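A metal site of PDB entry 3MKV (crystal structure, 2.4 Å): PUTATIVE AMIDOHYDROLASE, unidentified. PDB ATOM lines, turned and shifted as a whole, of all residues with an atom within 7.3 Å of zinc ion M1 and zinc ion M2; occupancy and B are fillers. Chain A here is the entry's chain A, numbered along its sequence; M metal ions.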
ATOM      1  N   HIS A  65     -17.048   6.353  -4.467  1.00  0.00           N
ATOM      2  CA  HIS A  65     -18.286   7.084  -4.200  1.00  0.00           C
ATOM      3  C   HIS A  65     -19.483   6.176  -4.005  1.00  0.00           C
ATOM      4  O   HIS A  65     -20.229   5.890  -4.924  1.00  0.00           O
ATOM      5  CB  HIS A  65     -18.576   8.119  -5.311  1.00  0.00           C
ATOM      6  CG  HIS A  65     -19.557   9.171  -4.906  1.00  0.00           C
ATOM      7  ND1 HIS A  65     -19.243  10.508  -4.922  1.00  0.00           N
ATOM      8  CD2 HIS A  65     -20.823   9.088  -4.458  1.00  0.00           C
ATOM      9  CE1 HIS A  65     -20.290  11.209  -4.499  1.00  0.00           C
ATOM     10  NE2 HIS A  65     -21.252  10.363  -4.211  1.00  0.00           N
ATOM     11  N   VAL A  66     -19.677   5.716  -2.782  1.00  0.00           N
ATOM     12  CA  VAL A  66     -20.869   4.954  -2.455  1.00  0.00           C
ATOM     13  C   VAL A  66     -21.595   5.609  -1.296  1.00  0.00           C
ATOM     14  O   VAL A  66     -21.029   6.440  -0.580  1.00  0.00           O
ATOM     15  CB  VAL A  66     -20.536   3.464  -2.091  1.00  0.00           C
ATOM     16  CG1 VAL A  66     -19.805   2.783  -3.228  1.00  0.00           C
ATOM     17  CG2 VAL A  66     -19.699   3.388  -0.834  1.00  0.00           C
ATOM     18  N   HIS A  67     -22.855   5.238  -1.129  1.00  0.00           N
ATOM     19  CA  HIS A  67     -23.600   5.550   0.085  1.00  0.00           C
ATOM     20  C   HIS A  67     -24.153   4.249   0.648  1.00  0.00           C
ATOM     21  O   HIS A  67     -25.114   3.689   0.139  1.00  0.00           O
ATOM     22  CB  HIS A  67     -24.710   6.543  -0.209  1.00  0.00           C
ATOM     23  CG  HIS A  67     -24.208   7.847  -0.747  1.00  0.00           C
ATOM     24  ND1 HIS A  67     -23.623   8.805   0.047  1.00  0.00           N
ATOM     25  CD2 HIS A  67     -24.192   8.341  -2.005  1.00  0.00           C
ATOM     26  CE1 HIS A  67     -23.277   9.837  -0.695  1.00  0.00           C
ATOM     27  NE2 HIS A  67     -23.609   9.582  -1.945  1.00  0.00           N
ATOM     28  N   ALA A 108     -19.359   8.475   0.476  1.00  0.00           N
ATOM     29  CA  ALA A 108     -19.421   9.889   0.166  1.00  0.00           C
ATOM     30  C   ALA A 108     -20.417  10.650   1.039  1.00  0.00           C
ATOM     31  O   ALA A 108     -20.608  11.850   0.868  1.00  0.00           O
ATOM     32  CB  ALA A 108     -19.737  10.076  -1.315  1.00  0.00           C
ATOM     33  N   GLY A 109     -21.053   9.957   1.982  1.00  0.00           N
ATOM     34  CA  GLY A 109     -21.978  10.613   2.885  1.00  0.00           C
ATOM     35  C   GLY A 109     -22.951   9.641   3.511  1.00  0.00           C
ATOM     36  O   GLY A 109     -23.651   8.890   2.806  1.00  0.00           O
ATOM     37  N   HIS A 142     -27.936  20.719  -1.775  1.00  0.00           N
ATOM     38  CA  HIS A 142     -28.159  19.328  -2.126  1.00  0.00           C
ATOM     39  C   HIS A 142     -28.581  18.508  -0.910  1.00  0.00           C
ATOM     40  O   HIS A 142     -29.626  17.873  -0.908  1.00  0.00           O
ATOM     41  CB  HIS A 142     -26.903  18.722  -2.753  1.00  0.00           C
ATOM     42  CG  HIS A 142     -27.163  17.509  -3.588  1.00  0.00           C
ATOM     43  ND1 HIS A 142     -28.031  17.523  -4.664  1.00  0.00           N
ATOM     44  CD2 HIS A 142     -26.665  16.253  -3.522  1.00  0.00           C
ATOM     45  CE1 HIS A 142     -28.055  16.325  -5.214  1.00  0.00           C
ATOM     46  NE2 HIS A 142     -27.247  15.532  -4.536  1.00  0.00           N
ATOM     47  N   LEU A 167     -27.629  11.213   5.228  1.00  0.00           N
ATOM     48  CA  LEU A 167     -26.450  11.318   4.375  1.00  0.00           C
ATOM     49  C   LEU A 167     -25.684  12.649   4.573  1.00  0.00           C
ATOM     50  O   LEU A 167     -24.471  12.729   4.329  1.00  0.00           O
ATOM     51  CB  LEU A 167     -26.835  11.193   2.899  1.00  0.00           C
ATOM     52  CG  LEU A 167     -27.525   9.968   2.284  1.00  0.00           C
ATOM     53  CD1 LEU A 167     -27.269   9.989   0.766  1.00  0.00           C
ATOM     54  CD2 LEU A 167     -27.095   8.624   2.868  1.00  0.00           C
ATOM     55  N   KCX A 193     -16.837  15.566   3.115  1.00  0.00           N
ATOM     56  CA  KCX A 193     -17.697  15.780   1.967  1.00  0.00           C
ATOM     57  CB  KCX A 193     -18.700  14.643   1.843  1.00  0.00           C
ATOM     58  CG  KCX A 193     -19.706  14.778   0.682  1.00  0.00           C
ATOM     59  CD  KCX A 193     -18.983  14.718  -0.662  1.00  0.00           C
ATOM     60  CE  KCX A 193     -19.954  14.640  -1.826  1.00  0.00           C
ATOM     61  NZ  KCX A 193     -21.013  13.638  -1.548  1.00  0.00           N
ATOM     62  C   KCX A 193     -18.461  17.102   2.067  1.00  0.00           C
ATOM     63  O   KCX A 193     -18.983  17.455   3.129  1.00  0.00           O
ATOM     64  CX  KCX A 193     -21.832  13.269  -2.533  1.00  0.00           C
ATOM     65  OQ1 KCX A 193     -21.706  13.758  -3.666  1.00  0.00           O
ATOM     66  OQ2 KCX A 193     -22.707  12.432  -2.302  1.00  0.00           O
ATOM     67  N   ILE A 194     -18.566  17.815   0.951  1.00  0.00           N
ATOM     68  CA  ILE A 194     -19.461  18.966   0.873  1.00  0.00           C
ATOM     69  C   ILE A 194     -20.241  18.897  -0.420  1.00  0.00           C
ATOM     70  O   ILE A 194     -19.758  18.330  -1.411  1.00  0.00           O
ATOM     71  CB  ILE A 194     -18.683  20.306   0.858  1.00  0.00           C
ATOM     72  CG1 ILE A 194     -17.891  20.454  -0.450  1.00  0.00           C
ATOM     73  CG2 ILE A 194     -17.792  20.411   2.074  1.00  0.00           C
ATOM     74  CD1 ILE A 194     -17.367  21.857  -0.742  1.00  0.00           C
ATOM     75  N   MET A 195     -21.438  19.463  -0.402  1.00  0.00           N
ATOM     76  CA  MET A 195     -22.159  19.725  -1.635  1.00  0.00           C
ATOM     77  C   MET A 195     -21.719  21.089  -2.139  1.00  0.00           C
ATOM     78  O   MET A 195     -21.937  22.114  -1.484  1.00  0.00           O
ATOM     79  CB  MET A 195     -23.675  19.682  -1.400  1.00  0.00           C
ATOM     80  CG  MET A 195     -24.182  18.367  -0.828  1.00  0.00           C
ATOM     81  SD  MET A 195     -23.472  16.877  -1.556  1.00  0.00           S
ATOM     82  CE  MET A 195     -24.400  15.627  -0.690  1.00  0.00           C
ATOM     83  N   GLY A 198     -25.922  22.199  -6.727  1.00  0.00           N
ATOM     84  CA  GLY A 198     -27.212  21.539  -6.704  1.00  0.00           C
ATOM     85  C   GLY A 198     -27.080  20.127  -7.250  1.00  0.00           C
ATOM     86  O   GLY A 198     -26.062  19.761  -7.839  1.00  0.00           O
ATOM     87  N   GLY A 199     -28.117  19.324  -7.048  1.00  0.00           N
ATOM     88  CA  GLY A 199     -28.083  17.933  -7.452  1.00  0.00           C
ATOM     89  C   GLY A 199     -29.426  17.442  -7.940  1.00  0.00           C
ATOM     90  O   GLY A 199     -30.405  18.183  -7.927  1.00  0.00           O
ATOM     91  N   ALA A 233     -15.966  17.121  -3.131  1.00  0.00           N
ATOM     92  CA  ALA A 233     -17.075  18.030  -3.335  1.00  0.00           C
ATOM     93  C   ALA A 233     -17.917  17.603  -4.496  1.00  0.00           C
ATOM     94  O   ALA A 233     -17.397  17.375  -5.578  1.00  0.00           O
ATOM     95  CB  ALA A 233     -16.558  19.439  -3.552  1.00  0.00           C
ATOM     96  N   HIS A 234     -19.209  17.507  -4.269  1.00  0.00           N
ATOM     97  CA  HIS A 234     -20.181  17.227  -5.311  1.00  0.00           C
ATOM     98  C   HIS A 234     -20.359  18.529  -6.111  1.00  0.00           C
ATOM     99  O   HIS A 234     -20.635  19.583  -5.535  1.00  0.00           O
ATOM    100  CB  HIS A 234     -21.469  16.738  -4.634  1.00  0.00           C
ATOM    101  CG  HIS A 234     -22.727  16.958  -5.426  1.00  0.00           C
ATOM    102  ND1 HIS A 234     -23.536  15.915  -5.834  1.00  0.00           N
ATOM    103  CD2 HIS A 234     -23.353  18.086  -5.820  1.00  0.00           C
ATOM    104  CE1 HIS A 234     -24.581  16.387  -6.479  1.00  0.00           C
ATOM    105  NE2 HIS A 234     -24.494  17.705  -6.491  1.00  0.00           N
ATOM    106  N   ALA A 235     -20.135  18.455  -7.423  1.00  0.00           N
ATOM    107  CA  ALA A 235     -20.204  19.627  -8.317  1.00  0.00           C
ATOM    108  C   ALA A 235     -20.422  19.211  -9.765  1.00  0.00           C
ATOM    109  O   ALA A 235     -19.728  18.323 -10.268  1.00  0.00           O
ATOM    110  CB  ALA A 235     -18.939  20.470  -8.192  1.00  0.00           C
ATOM    111  N   TYR A 236     -21.357  19.849 -10.456  1.00  0.00           N
ATOM    112  CA  TYR A 236     -21.681  19.489 -11.847  1.00  0.00           C
ATOM    113  C   TYR A 236     -21.126  20.433 -12.924  1.00  0.00           C
ATOM    114  O   TYR A 236     -20.526  19.973 -13.905  1.00  0.00           O
ATOM    115  CB  TYR A 236     -23.183  19.331 -12.034  1.00  0.00           C
ATOM    116  CG  TYR A 236     -23.751  18.053 -11.448  1.00  0.00           C
ATOM    117  CD1 TYR A 236     -23.228  16.817 -11.809  1.00  0.00           C
ATOM    118  CD2 TYR A 236     -24.824  18.083 -10.574  1.00  0.00           C
ATOM    119  CE1 TYR A 236     -23.744  15.640 -11.288  1.00  0.00           C
ATOM    120  CE2 TYR A 236     -25.351  16.921 -10.041  1.00  0.00           C
ATOM    121  CZ  TYR A 236     -24.805  15.692 -10.399  1.00  0.00           C
ATOM    122  OH  TYR A 236     -25.321  14.528  -9.879  1.00  0.00           O
ATOM    123  N   GLU A 253     -16.706  15.352  -7.541  1.00  0.00           N
ATOM    124  CA  GLU A 253     -17.591  14.219  -7.690  1.00  0.00           C
ATOM    125  C   GLU A 253     -18.585  14.470  -8.822  1.00  0.00           C
ATOM    126  O   GLU A 253     -19.260  15.503  -8.860  1.00  0.00           O
ATOM    127  CB  GLU A 253     -18.321  13.922  -6.377  1.00  0.00           C
ATOM    128  CG  GLU A 253     -17.411  13.770  -5.165  1.00  0.00           C
ATOM    129  CD  GLU A 253     -16.372  12.669  -5.312  1.00  0.00           C
ATOM    130  OE1 GLU A 253     -16.759  11.488  -5.465  1.00  0.00           O
ATOM    131  OE2 GLU A 253     -15.152  12.988  -5.254  1.00  0.00           O
ATOM    132  N   HIS A 254     -18.653  13.504  -9.734  1.00  0.00           N
ATOM    133  CA  HIS A 254     -19.554  13.583 -10.879  1.00  0.00           C
ATOM    134  C   HIS A 254     -18.890  14.388 -11.997  1.00  0.00           C
ATOM    135  O   HIS A 254     -18.324  13.804 -12.927  1.00  0.00           O
ATOM    136  CB  HIS A 254     -20.904  14.185 -10.475  1.00  0.00           C
ATOM    137  CG  HIS A 254     -21.518  13.522  -9.280  1.00  0.00           C
ATOM    138  ND1 HIS A 254     -21.752  12.167  -9.212  1.00  0.00           N
ATOM    139  CD2 HIS A 254     -21.975  14.040  -8.114  1.00  0.00           C
ATOM    140  CE1 HIS A 254     -22.312  11.876  -8.053  1.00  0.00           C
ATOM    141  NE2 HIS A 254     -22.453  12.994  -7.375  1.00  0.00           N
ATOM    142  N   THR A 276     -19.694   9.287 -11.897  1.00  0.00           N
ATOM    143  CA  THR A 276     -20.569   8.265 -11.336  1.00  0.00           C
ATOM    144  C   THR A 276     -21.710   7.937 -12.294  1.00  0.00           C
ATOM    145  O   THR A 276     -22.888   7.960 -11.912  1.00  0.00           O
ATOM    146  CB  THR A 276     -21.097   8.690  -9.945  1.00  0.00           C
ATOM    147  OG1 THR A 276     -21.829   9.915 -10.055  1.00  0.00           O
ATOM    148  CG2 THR A 276     -19.927   8.891  -8.974  1.00  0.00           C
ATOM    149  N   TYR A 280     -26.883   7.624 -13.042  1.00  0.00           N
ATOM    150  CA  TYR A 280     -27.819   8.383 -13.879  1.00  0.00           C
ATOM    151  C   TYR A 280     -28.641   7.474 -14.786  1.00  0.00           C
ATOM    152  O   TYR A 280     -29.858   7.666 -14.918  1.00  0.00           O
ATOM    153  CB  TYR A 280     -27.075   9.473 -14.647  1.00  0.00           C
ATOM    154  CG  TYR A 280     -26.218  10.284 -13.711  1.00  0.00           C
ATOM    155  CD1 TYR A 280     -26.789  10.945 -12.629  1.00  0.00           C
ATOM    156  CD2 TYR A 280     -24.832  10.371 -13.870  1.00  0.00           C
ATOM    157  CE1 TYR A 280     -26.023  11.668 -11.742  1.00  0.00           C
ATOM    158  CE2 TYR A 280     -24.056  11.101 -12.976  1.00  0.00           C
ATOM    159  CZ  TYR A 280     -24.670  11.754 -11.913  1.00  0.00           C
ATOM    160  OH  TYR A 280     -23.939  12.480 -10.995  1.00  0.00           O
ATOM    161  N   THR A 325     -19.649   5.084  -8.316  1.00  0.00           N
ATOM    162  CA  THR A 325     -20.944   4.589  -8.765  1.00  0.00           C
ATOM    163  C   THR A 325     -22.117   5.465  -8.289  1.00  0.00           C
ATOM    164  O   THR A 325     -22.972   5.828  -9.106  1.00  0.00           O
ATOM    165  CB  THR A 325     -21.150   3.091  -8.380  1.00  0.00           C
ATOM    166  OG1 THR A 325     -21.055   2.931  -6.952  1.00  0.00           O
ATOM    167  CG2 THR A 325     -20.106   2.191  -9.067  1.00  0.00           C
ATOM    168  N   ASP A 326     -22.161   5.763  -6.996  1.00  0.00           N
ATOM    169  CA  ASP A 326     -23.193   6.640  -6.415  1.00  0.00           C
ATOM    170  C   ASP A 326     -24.617   6.127  -6.595  1.00  0.00           C
ATOM    171  O   ASP A 326     -25.529   6.887  -6.937  1.00  0.00           O
ATOM    172  CB  ASP A 326     -23.089   8.065  -6.993  1.00  0.00           C
ATOM    173  CG  ASP A 326     -23.895   9.085  -6.208  1.00  0.00           C
ATOM    174  OD1 ASP A 326     -24.177   8.852  -5.010  1.00  0.00           O
ATOM    175  OD2 ASP A 326     -24.270  10.138  -6.794  1.00  0.00           O
ATOM    176  N   LEU A 327     -24.832   4.838  -6.340  1.00  0.00           N
ATOM    177  CA  LEU A 327     -26.142   4.215  -6.544  1.00  0.00           C
ATOM    178  C   LEU A 327     -27.021   4.214  -5.275  1.00  0.00           C
ATOM    179  O   LEU A 327     -26.499   4.243  -4.155  1.00  0.00           O
ATOM    180  CB  LEU A 327     -25.963   2.790  -7.082  1.00  0.00           C
ATOM    181  CG  LEU A 327     -25.415   2.666  -8.515  1.00  0.00           C
ATOM    182  CD1 LEU A 327     -24.759   1.326  -8.760  1.00  0.00           C
ATOM    183  CD2 LEU A 327     -26.508   2.934  -9.558  1.00  0.00           C
ATOM    184  N   LEU A 328     -28.336   4.147  -5.462  1.00  0.00           N
ATOM    185  CA  LEU A 328     -29.298   4.223  -4.364  1.00  0.00           C
ATOM    186  C   LEU A 328     -30.218   3.008  -4.318  1.00  0.00           C
ATOM    187  O   LEU A 328     -30.511   2.404  -5.341  1.00  0.00           O
ATOM    188  CB  LEU A 328     -30.154   5.486  -4.472  1.00  0.00           C
ATOM    189  CG  LEU A 328     -29.447   6.805  -4.810  1.00  0.00           C
ATOM    190  CD1 LEU A 328     -30.464   7.897  -5.098  1.00  0.00           C
ATOM    191  CD2 LEU A 328     -28.492   7.248  -3.694  1.00  0.00           C
HETATM  192 ZN    ZN M   1     -23.296  13.608  -5.155  1.00  0.00          ZN
HETATM  193 ZN    ZN M   2     -23.234  10.624  -3.709  1.00  0.00          ZN
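OQ1 of KCX 193 binds zinc ion M1. A ring nitrogen (ND1) of His 234 binds zinc ion M1 (2.4 Å). Zinc ion M1 is bound by NE2 of His 254 (2.5 Å). Zinc ion M1 has three donor atoms within binding distance.
Zinc ion M2 is bound by NE2 of His 65 (2.1 Å), NE2 of His 67 (2.1 Å), OQ2 of KCX 193 (2.4 Å) and OD1 of Asp 326 (2.4 Å).
OE1 of Glu 253 is in hydrogen-bond range of ND1 of His 65. A ring nitrogen (ND1) of His 67 sits at hydrogen-bond distance from the backbone carbonyl oxygen (O) of Gly 109 (2.8 Å). The side-chain carboxylate of Asp 326 lies close to a ring nitrogen (NE2) of His 254 (3.4 Å). OH of Tyr 280 is in hydrogen-bond range of ND1 of His 254 (2.8 Å). A ring nitrogen (ND1) of His 254 lies within hydrogen-bond range of the side-chain hydroxyl (OG1) of Thr 276 (2.4 Å). NZ of KCX 193 sits at hydrogen-bond distance from O of Ala 108, 3.0 Å away. O of Gly 198 sits at hydrogen-bond distance from NE2 of His 234, 2.9 Å away. O of Ile 194 lies within hydrogen-bond range of N of His 234, 3.0 Å away.
Five residues have an atom within 4 Å of zinc ion M1: His 65, KCX 193, His 234, His 254 and Asp 326.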
